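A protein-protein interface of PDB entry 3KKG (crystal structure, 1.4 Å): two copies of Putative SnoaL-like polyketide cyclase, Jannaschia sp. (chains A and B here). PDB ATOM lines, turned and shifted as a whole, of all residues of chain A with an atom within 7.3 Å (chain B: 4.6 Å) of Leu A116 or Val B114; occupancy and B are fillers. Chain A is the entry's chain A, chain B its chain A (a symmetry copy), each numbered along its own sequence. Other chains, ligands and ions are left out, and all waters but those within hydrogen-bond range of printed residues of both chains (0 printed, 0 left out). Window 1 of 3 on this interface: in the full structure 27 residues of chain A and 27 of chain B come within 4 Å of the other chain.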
ATOM      1  N   PHE A  19      10.866 -35.399   7.182  1.00  0.00           N
ATOM      2  CA  PHE A  19      11.583 -36.285   6.288  1.00  0.00           C
ATOM      3  C   PHE A  19      10.661 -37.339   5.653  1.00  0.00           C
ATOM      4  O   PHE A  19      11.145 -38.179   4.900  1.00  0.00           O
ATOM      5  CB  PHE A  19      12.781 -36.943   6.985  1.00  0.00           C
ATOM      6  CG  PHE A  19      13.831 -35.922   7.377  1.00  0.00           C
ATOM      7  CD1 PHE A  19      13.699 -35.177   8.539  1.00  0.00           C
ATOM      8  CD2 PHE A  19      14.833 -35.612   6.492  1.00  0.00           C
ATOM      9  CE1 PHE A  19      14.629 -34.204   8.837  1.00  0.00           C
ATOM     10  CE2 PHE A  19      15.790 -34.628   6.808  1.00  0.00           C
ATOM     11  CZ  PHE A  19      15.648 -33.924   7.966  1.00  0.00           C
ATOM     12  N   ARG A  42      13.122 -19.541  10.607  1.00  0.00           N
ATOM     13  CA  ARG A  42      14.259 -19.094   9.782  1.00  0.00           C
ATOM     14  C   ARG A  42      14.961 -20.328   9.201  1.00  0.00           C
ATOM     15  O   ARG A  42      15.260 -21.276   9.924  1.00  0.00           O
ATOM     16  CB  ARG A  42      15.330 -18.413  10.658  1.00  0.00           C
ATOM     17  CG  ARG A  42      14.943 -17.093  11.210  1.00  0.00           C
ATOM     18  CD  ARG A  42      15.743 -16.741  12.475  1.00  0.00           C
ATOM     19  NE  ARG A  42      17.180 -16.921  12.296  1.00  0.00           N
ATOM     20  CZ  ARG A  42      18.030 -16.016  11.816  1.00  0.00           C
ATOM     21  NH1 ARG A  42      17.639 -14.821  11.439  1.00  0.00           N
ATOM     22  NH2 ARG A  42      19.310 -16.318  11.726  1.00  0.00           N
ATOM     23  N   ILE A  44      18.287 -21.566   6.872  1.00  0.00           N
ATOM     24  CA  ILE A  44      19.647 -21.176   6.564  1.00  0.00           C
ATOM     25  C   ILE A  44      20.219 -22.278   5.662  1.00  0.00           C
ATOM     26  O   ILE A  44      20.265 -23.458   6.078  1.00  0.00           O
ATOM     27  CB  ILE A  44      20.493 -21.033   7.844  1.00  0.00           C
ATOM     28  CG1 ILE A  44      19.985 -19.848   8.681  1.00  0.00           C
ATOM     29  CG2 ILE A  44      21.994 -20.850   7.502  1.00  0.00           C
ATOM     30  CD1 ILE A  44      20.588 -19.772  10.088  1.00  0.00           C
ATOM     31  N   ASN A  84      17.874 -29.145  20.381  1.00  0.00           N
ATOM     32  CA  ASN A  84      18.670 -29.258  19.163  1.00  0.00           C
ATOM     33  C   ASN A  84      18.588 -30.655  18.637  1.00  0.00           C
ATOM     34  O   ASN A  84      18.889 -31.587  19.347  1.00  0.00           O
ATOM     35  CB  ASN A  84      20.143 -28.954  19.432  1.00  0.00           C
ATOM     36  CG  ASN A  84      20.344 -27.504  19.896  1.00  0.00           C
ATOM     37  OD1 ASN A  84      20.442 -26.606  19.078  1.00  0.00           O
ATOM     38  ND2 ASN A  84      20.295 -27.283  21.179  1.00  0.00           N
ATOM     39  N   VAL A  85      18.109 -30.802  17.378  1.00  0.00           N
ATOM     40  CA  VAL A  85      18.009 -32.084  16.711  1.00  0.00           C
ATOM     41  C   VAL A  85      18.829 -32.014  15.435  1.00  0.00           C
ATOM     42  O   VAL A  85      18.651 -31.091  14.609  1.00  0.00           O
ATOM     43  CB  VAL A  85      16.554 -32.450  16.367  1.00  0.00           C
ATOM     44  CG1 VAL A  85      16.556 -33.797  15.678  1.00  0.00           C
ATOM     45  CG2 VAL A  85      15.697 -32.498  17.641  1.00  0.00           C
ATOM     46  N   VAL A  86      19.690 -33.000  15.252  1.00  0.00           N
ATOM     47  CA  VAL A  86      20.571 -33.078  14.097  1.00  0.00           C
ATOM     48  C   VAL A  86      20.251 -34.335  13.348  1.00  0.00           C
ATOM     49  O   VAL A  86      20.194 -35.419  13.922  1.00  0.00           O
ATOM     50  CB  VAL A  86      22.069 -33.107  14.544  1.00  0.00           C
ATOM     51  CG1 VAL A  86      23.003 -33.210  13.309  1.00  0.00           C
ATOM     52  CG2 VAL A  86      22.386 -31.896  15.467  1.00  0.00           C
ATOM     53  N   VAL A  87      19.915 -34.221  12.078  1.00  0.00           N
ATOM     54  CA  VAL A  87      19.542 -35.323  11.222  1.00  0.00           C
ATOM     55  C   VAL A  87      20.554 -35.431  10.101  1.00  0.00           C
ATOM     56  O   VAL A  87      20.701 -34.503   9.317  1.00  0.00           O
ATOM     57  CB  VAL A  87      18.111 -35.175  10.665  1.00  0.00           C
ATOM     58  CG1 VAL A  87      17.770 -36.380   9.791  1.00  0.00           C
ATOM     59  CG2 VAL A  87      17.100 -35.014  11.793  1.00  0.00           C
ATOM     60  N   VAL A 114      23.283 -32.945   6.150  1.00  0.00           N
ATOM     61  CA  VAL A 114      23.007 -32.754   7.591  1.00  0.00           C
ATOM     62  C   VAL A 114      22.107 -31.549   7.757  1.00  0.00           C
ATOM     63  O   VAL A 114      22.275 -30.503   7.127  1.00  0.00           O
ATOM     64  CB  VAL A 114      24.291 -32.618   8.391  1.00  0.00           C
ATOM     65  CG1 VAL A 114      25.127 -31.453   7.957  1.00  0.00           C
ATOM     66  CG2 VAL A 114      23.927 -32.493   9.897  1.00  0.00           C
ATOM     67  N   THR A 115      21.022 -31.717   8.535  1.00  0.00           N
ATOM     68  CA  THR A 115      20.065 -30.664   8.859  1.00  0.00           C
ATOM     69  C   THR A 115      20.092 -30.471  10.350  1.00  0.00           C
ATOM     70  O   THR A 115      19.957 -31.476  11.089  1.00  0.00           O
ATOM     71  CB  THR A 115      18.653 -31.011   8.324  1.00  0.00           C
ATOM     72  OG1 THR A 115      18.779 -31.540   6.974  1.00  0.00           O
ATOM     73  CG2 THR A 115      17.741 -29.826   8.327  1.00  0.00           C
ATOM     74  N   LEU A 116      20.207 -29.227  10.785  1.00  0.00           N
ATOM     75  CA  LEU A 116      20.384 -28.905  12.190  1.00  0.00           C
ATOM     76  C   LEU A 116      19.194 -28.063  12.602  1.00  0.00           C
ATOM     77  O   LEU A 116      19.051 -26.897  12.156  1.00  0.00           O
ATOM     78  CB  LEU A 116      21.716 -28.167  12.367  1.00  0.00           C
ATOM     79  CG  LEU A 116      22.909 -28.973  11.824  1.00  0.00           C
ATOM     80  CD1 LEU A 116      23.626 -28.208  10.762  1.00  0.00           C
ATOM     81  CD2 LEU A 116      23.842 -29.359  12.915  1.00  0.00           C
ATOM     82  N   PHE A 117      18.329 -28.608  13.443  1.00  0.00           N
ATOM     83  CA  PHE A 117      17.097 -27.954  13.852  1.00  0.00           C
ATOM     84  C   PHE A 117      17.223 -27.398  15.255  1.00  0.00           C
ATOM     85  O   PHE A 117      17.850 -28.029  16.134  1.00  0.00           O
ATOM     86  CB  PHE A 117      15.955 -28.994  13.863  1.00  0.00           C
ATOM     87  CG  PHE A 117      15.632 -29.531  12.492  1.00  0.00           C
ATOM     88  CD1 PHE A 117      14.686 -28.917  11.705  1.00  0.00           C
ATOM     89  CD2 PHE A 117      16.213 -30.699  12.019  1.00  0.00           C
ATOM     90  CE1 PHE A 117      14.366 -29.422  10.445  1.00  0.00           C
ATOM     91  CE2 PHE A 117      15.874 -31.206  10.760  1.00  0.00           C
ATOM     92  CZ  PHE A 117      14.913 -30.585   9.992  1.00  0.00           C
ATOM     93  N   THR A 118      16.575 -26.265  15.477  1.00  0.00           N
ATOM     94  CA  THR A 118      16.349 -25.731  16.820  1.00  0.00           C
ATOM     95  C   THR A 118      14.850 -25.635  17.027  1.00  0.00           C
ATOM     96  O   THR A 118      14.105 -25.192  16.127  1.00  0.00           O
ATOM     97  CB  THR A 118      16.969 -24.346  16.962  1.00  0.00           C
ATOM     98  OG1 THR A 118      18.348 -24.428  16.571  1.00  0.00           O
ATOM     99  CG2 THR A 118      16.921 -23.843  18.405  1.00  0.00           C
ATOM    100  N   VAL A 124       9.458 -26.017  15.554  1.00  0.00           N
ATOM    101  CA  VAL A 124      10.737 -25.746  14.934  1.00  0.00           C
ATOM    102  C   VAL A 124      10.869 -24.252  14.634  1.00  0.00           C
ATOM    103  O   VAL A 124      10.007 -23.647  13.941  1.00  0.00           O
ATOM    104  CB  VAL A 124      10.902 -26.562  13.642  1.00  0.00           C
ATOM    105  CG1 VAL A 124      12.200 -26.204  12.925  1.00  0.00           C
ATOM    106  CG2 VAL A 124      10.836 -28.060  13.908  1.00  0.00           C
ATOM    107  N   GLU A 126      14.187 -22.837  13.727  1.00  0.00           N
ATOM    108  CA  GLU A 126      15.311 -22.607  12.825  1.00  0.00           C
ATOM    109  C   GLU A 126      15.803 -23.942  12.282  1.00  0.00           C
ATOM    110  O   GLU A 126      15.769 -24.979  12.980  1.00  0.00           O
ATOM    111  CB  GLU A 126      16.460 -21.911  13.546  1.00  0.00           C
ATOM    112  CG  GLU A 126      17.613 -21.535  12.603  1.00  0.00           C
ATOM    113  CD  GLU A 126      18.650 -20.658  13.254  1.00  0.00           C
ATOM    114  OE1 GLU A 126      18.371 -19.465  13.438  1.00  0.00           O
ATOM    115  OE2 GLU A 126      19.694 -21.241  13.650  1.00  0.00           O
ATOM    116  N   MET A 127      16.237 -23.907  11.033  1.00  0.00           N
ATOM    117  CA  MET A 127      16.784 -25.035  10.340  1.00  0.00           C
ATOM    118  C   MET A 127      18.027 -24.584   9.588  1.00  0.00           C
ATOM    119  O   MET A 127      17.925 -23.639   8.813  1.00  0.00           O
ATOM    120  CB  MET A 127      15.754 -25.578   9.348  1.00  0.00           C
ATOM    121  CG  MET A 127      16.186 -26.780   8.565  1.00  0.00           C
ATOM    122  SD  MET A 127      14.757 -27.368   7.414  1.00  0.00           S
ATOM    123  CE  MET A 127      14.905 -26.013   6.191  1.00  0.00           C
ATOM    124  N   ARG A 128      19.171 -25.204   9.865  1.00  0.00           N
ATOM    125  CA  ARG A 128      20.408 -24.964   9.153  1.00  0.00           C
ATOM    126  C   ARG A 128      20.737 -26.195   8.345  1.00  0.00           C
ATOM    127  O   ARG A 128      20.472 -27.316   8.767  1.00  0.00           O
ATOM    128  CB  ARG A 128      21.567 -24.684  10.121  1.00  0.00           C
ATOM    129  CG  ARG A 128      21.355 -23.500  11.001  1.00  0.00           C
ATOM    130  CD  ARG A 128      22.423 -23.419  12.096  1.00  0.00           C
ATOM    131  NE  ARG A 128      22.243 -22.238  12.920  1.00  0.00           N
ATOM    132  CZ  ARG A 128      23.219 -21.791  13.702  1.00  0.00           C
ATOM    133  NH1 ARG A 128      24.406 -22.383  13.735  1.00  0.00           N
ATOM    134  NH2 ARG A 128      23.003 -20.719  14.464  1.00  0.00           N
ATOM    135  N   TYR A 129      21.258 -26.023   7.148  1.00  0.00           N
ATOM    136  CA  TYR A 129      21.458 -27.101   6.220  1.00  0.00           C
ATOM    137  C   TYR A 129      22.827 -27.083   5.575  1.00  0.00           C
ATOM    138  O   TYR A 129      23.288 -26.068   5.080  1.00  0.00           O
ATOM    139  CB  TYR A 129      20.356 -27.035   5.127  1.00  0.00           C
ATOM    140  CG  TYR A 129      20.423 -28.203   4.191  1.00  0.00           C
ATOM    141  CD1 TYR A 129      19.967 -29.442   4.601  1.00  0.00           C
ATOM    142  CD2 TYR A 129      20.932 -28.094   2.924  1.00  0.00           C
ATOM    143  CE1 TYR A 129      20.079 -30.533   3.800  1.00  0.00           C
ATOM    144  CE2 TYR A 129      21.024 -29.196   2.099  1.00  0.00           C
ATOM    145  CZ  TYR A 129      20.581 -30.403   2.532  1.00  0.00           C
ATOM    146  OH  TYR A 129      20.684 -31.521   1.728  1.00  0.00           O
ATOM    147  N   PHE A 130      23.374 -28.298   5.396  1.00  0.00           N
ATOM    148  CA  PHE A 130      24.524 -28.501   4.525  1.00  0.00           C
ATOM    149  C   PHE A 130      24.420 -29.795   3.766  1.00  0.00           C
ATOM    150  O   PHE A 130      24.070 -30.829   4.344  1.00  0.00           O
ATOM    151  CB  PHE A 130      25.837 -28.613   5.284  1.00  0.00           C
ATOM    152  CG  PHE A 130      26.195 -27.436   6.130  1.00  0.00           C
ATOM    153  CD1 PHE A 130      25.737 -27.310   7.415  1.00  0.00           C
ATOM    154  CD2 PHE A 130      27.085 -26.465   5.673  1.00  0.00           C
ATOM    155  CE1 PHE A 130      26.105 -26.199   8.212  1.00  0.00           C
ATOM    156  CE2 PHE A 130      27.474 -25.393   6.451  1.00  0.00           C
ATOM    157  CZ  PHE A 130      26.991 -25.257   7.687  1.00  0.00           C
ATOM    158  N   VAL B  86      28.300 -33.343  17.880  1.00  0.00           N
ATOM    159  CA  VAL B  86      28.154 -32.459  16.734  1.00  0.00           C
ATOM    160  C   VAL B  86      28.582 -31.084  17.144  1.00  0.00           C
ATOM    161  O   VAL B  86      28.133 -30.555  18.156  1.00  0.00           O
ATOM    162  CB  VAL B  86      26.666 -32.418  16.252  1.00  0.00           C
ATOM    163  CG1 VAL B  86      26.513 -31.460  15.042  1.00  0.00           C
ATOM    164  CG2 VAL B  86      26.142 -33.858  15.980  1.00  0.00           C
ATOM    165  N   VAL B  87      29.544 -30.511  16.449  1.00  0.00           N
ATOM    166  CA  VAL B  87      30.101 -29.209  16.730  1.00  0.00           C
ATOM    167  C   VAL B  87      29.823 -28.297  15.554  1.00  0.00           C
ATOM    168  O   VAL B  87      30.279 -28.564  14.450  1.00  0.00           O
ATOM    169  CB  VAL B  87      31.611 -29.269  17.039  1.00  0.00           C
ATOM    170  CG1 VAL B  87      32.132 -27.868  17.351  1.00  0.00           C
ATOM    171  CG2 VAL B  87      31.896 -30.227  18.189  1.00  0.00           C
ATOM    172  N   GLN B  88      29.122 -27.202  15.770  1.00  0.00           N
ATOM    173  CA  GLN B  88      28.992 -26.175  14.732  1.00  0.00           C
ATOM    174  C   GLN B  88      29.922 -25.032  15.085  1.00  0.00           C
ATOM    175  O   GLN B  88      30.034 -24.642  16.257  1.00  0.00           O
ATOM    176  CB  GLN B  88      27.605 -25.644  14.714  1.00  0.00           C
ATOM    177  CG  GLN B  88      26.515 -26.665  14.276  1.00  0.00           C
ATOM    178  CD  GLN B  88      25.193 -25.992  14.114  1.00  0.00           C
ATOM    179  OE1 GLN B  88      25.031 -25.198  13.208  1.00  0.00           O
ATOM    180  NE2 GLN B  88      24.273 -26.277  14.978  1.00  0.00           N
ATOM    181  N   ASP B 113      30.294 -23.975   9.696  1.00  0.00           N
ATOM    182  CA  ASP B 113      30.589 -25.356   9.394  1.00  0.00           C
ATOM    183  C   ASP B 113      29.922 -26.248  10.404  1.00  0.00           C
ATOM    184  O   ASP B 113      29.305 -25.784  11.385  1.00  0.00           O
ATOM    185  CB  ASP B 113      32.050 -25.583   9.221  1.00  0.00           C
ATOM    186  CG  ASP B 113      32.841 -25.638  10.470  1.00  0.00           C
ATOM    187  OD1 ASP B 113      32.302 -25.513  11.581  1.00  0.00           O
ATOM    188  OD2 ASP B 113      34.092 -25.768  10.356  1.00  0.00           O
ATOM    189  N   VAL B 114      30.061 -27.531  10.206  1.00  0.00           N
ATOM    190  CA  VAL B 114      29.574 -28.558  11.154  1.00  0.00           C
ATOM    191  C   VAL B 114      30.458 -29.781  11.041  1.00  0.00           C
ATOM    192  O   VAL B 114      30.838 -30.229   9.956  1.00  0.00           O
ATOM    193  CB  VAL B 114      28.113 -28.890  10.915  1.00  0.00           C
ATOM    194  CG1 VAL B 114      27.853 -29.422   9.538  1.00  0.00           C
ATOM    195  CG2 VAL B 114      27.653 -29.916  11.987  1.00  0.00           C
ATOM    196  N   THR B 115      30.926 -30.290  12.196  1.00  0.00           N
ATOM    197  CA  THR B 115      31.747 -31.492  12.299  1.00  0.00           C
ATOM    198  C   THR B 115      30.983 -32.493  13.119  1.00  0.00           C
ATOM    199  O   THR B 115      30.526 -32.135  14.232  1.00  0.00           O
ATOM    200  CB  THR B 115      33.140 -31.165  12.894  1.00  0.00           C
ATOM    201  OG1 THR B 115      33.643 -29.948  12.275  1.00  0.00           O
ATOM    202  CG2 THR B 115      34.115 -32.282  12.695  1.00  0.00           C
ATOM    203  N   LEU B 116      30.887 -33.716  12.624  1.00  0.00           N
ATOM    204  CA  LEU B 116      30.066 -34.744  13.238  1.00  0.00           C
ATOM    205  C   LEU B 116      30.995 -35.870  13.640  1.00  0.00           C
ATOM    206  O   LEU B 116      31.560 -36.575  12.765  1.00  0.00           O
ATOM    207  CB  LEU B 116      28.997 -35.193  12.235  1.00  0.00           C
ATOM    208  CG  LEU B 116      28.138 -34.020  11.729  1.00  0.00           C
ATOM    209  CD1 LEU B 116      28.234 -33.895  10.245  1.00  0.00           C
ATOM    210  CD2 LEU B 116      26.722 -34.165  12.154  1.00  0.00           C
ATOM    211  N   ARG B 128      32.963 -36.599  10.284  1.00  0.00           N
ATOM    212  CA  ARG B 128      32.347 -36.159   9.049  1.00  0.00           C
ATOM    213  C   ARG B 128      32.270 -34.653   9.069  1.00  0.00           C
ATOM    214  O   ARG B 128      32.066 -34.044  10.115  1.00  0.00           O
ATOM    215  CB  ARG B 128      30.928 -36.724   8.899  1.00  0.00           C
ATOM    216  CG  ARG B 128      30.861 -38.213   8.891  1.00  0.00           C
ATOM    217  CD  ARG B 128      29.414 -38.709   8.982  1.00  0.00           C
ATOM    218  NE  ARG B 128      29.351 -40.158   8.924  1.00  0.00           N
ATOM    219  CZ  ARG B 128      28.210 -40.784   8.655  1.00  0.00           C
ATOM    220  NH1 ARG B 128      27.096 -40.113   8.395  1.00  0.00           N
ATOM    221  NH2 ARG B 128      28.188 -42.117   8.638  1.00  0.00           N
ATOM    222  N   TYR B 129      32.491 -34.011   7.941  1.00  0.00           N
ATOM    223  CA  TYR B 129      32.612 -32.581   7.864  1.00  0.00           C
ATOM    224  C   TYR B 129      31.811 -31.978   6.731  1.00  0.00           C
ATOM    225  O   TYR B 129      31.870 -32.423   5.597  1.00  0.00           O
ATOM    226  CB  TYR B 129      34.112 -32.211   7.708  1.00  0.00           C
ATOM    227  CG  TYR B 129      34.332 -30.730   7.747  1.00  0.00           C
ATOM    228  CD1 TYR B 129      34.272 -30.055   8.953  1.00  0.00           C
ATOM    229  CD2 TYR B 129      34.589 -30.000   6.616  1.00  0.00           C
ATOM    230  CE1 TYR B 129      34.398 -28.704   9.010  1.00  0.00           C
ATOM    231  CE2 TYR B 129      34.741 -28.630   6.675  1.00  0.00           C
ATOM    232  CZ  TYR B 129      34.665 -27.993   7.869  1.00  0.00           C
ATOM    233  OH  TYR B 129      34.793 -26.620   7.946  1.00  0.00           O
ATOM    234  N   PHE B 130      31.226 -30.803   7.026  1.00  0.00           N
ATOM    235  CA  PHE B 130      30.685 -29.934   5.991  1.00  0.00           C
ATOM    236  C   PHE B 130      30.931 -28.484   6.303  1.00  0.00           C
ATOM    237  O   PHE B 130      30.733 -28.050   7.442  1.00  0.00           O
ATOM    238  CB  PHE B 130      29.174 -30.038   5.850  1.00  0.00           C
ATOM    239  CG  PHE B 130      28.650 -31.399   5.528  1.00  0.00           C
ATOM    240  CD1 PHE B 130      28.384 -32.317   6.509  1.00  0.00           C
ATOM    241  CD2 PHE B 130      28.323 -31.752   4.220  1.00  0.00           C
ATOM    242  CE1 PHE B 130      27.864 -33.594   6.188  1.00  0.00           C
ATOM    243  CE2 PHE B 130      27.788 -32.983   3.897  1.00  0.00           C
ATOM    244  CZ  PHE B 130      27.570 -33.886   4.855  1.00  0.00           C
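The guanidinium group of Arg A128 is in hydrogen-bond range of the side-chain amide oxygen of Gln B88 (2.9 Å).
OE2 of Glu A126 lies within salt-bridge range of NE of Arg A128. The side-chain hydroxyl (OH) of Tyr B129 lies within hydrogen-bond range of the side-chain carboxylate (OD2) of Asp B113 (2.7 Å). The backbone NH (N) of Leu A116 is in hydrogen-bond range of the backbone carbonyl oxygen (O) of Arg A128 (2.8 Å). N of Val B114 is in hydrogen-bond range of O of Phe B130, at 2.9 Å. O of Arg B128 is in hydrogen-bond range of N of Leu B116 (2.8 Å). O of Phe A130 is in hydrogen-bond range of N of Val A114 (2.9 Å).
Val A114 touches Val B114. Val A114 touches Leu B116 (CG2 to CD2, 3.96 Å). Val A114 touches Phe B130 (CG1 to CD1, 3.7 Å). CD2 of Leu A116 touches NE2 of Gln B88, at 3.7 Å. Leu A116 touches Val B114 (CD2 to CG2, 3.96 Å). Phe A130 touches Asp B113 (CZ to CA, 3.98 Å). Phe A130 touches Val B114. CB of Phe A130 touches CB of Phe B130, 3.7 Å away.
Of chain A, only Val A114 (3.7 Å), Leu A116 (3.96 Å) and Phe A130 (3.7 Å) come within 4 Å of Val B114. Of the printed residues of chain A, Leu B116 touches Val A114 (3.96 Å). Of the printed residues of chain A, Gln B88 touches Leu A116 and Arg A128. Of the printed residues of chain B, Val A114 touches Val B114, Leu B116 and Phe B130. Met A127 touches none of the printed residues of chain B. The nearest printed residue of chain B that does not touch Leu A116 is Val B86 (4.01 Å). The nearest residue of chain A that does not touch Val B114 is Val A86 (5.8 Å).
Along chain B the printed residues that touch a printed residue of chain A span positions 88 to 130. Hydrophobic or aromatic side chains of chain A within 4 Å of the printed part of chain B: Val A114, Leu A116 and Phe A130.
Val B114 touches its own counterpart, Val A114. Val A114 touches Leu B116, and with the chains exchanged Leu A116 touches Val B114. Val A114 touches Phe B130, and with the chains exchanged Phe A130 touches Val B114. Phe A130 touches its own counterpart, Phe B130. Of the 9 pairs that touch across the chains among the printed residues, 6 have their exchanged pair printed and touching as well.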
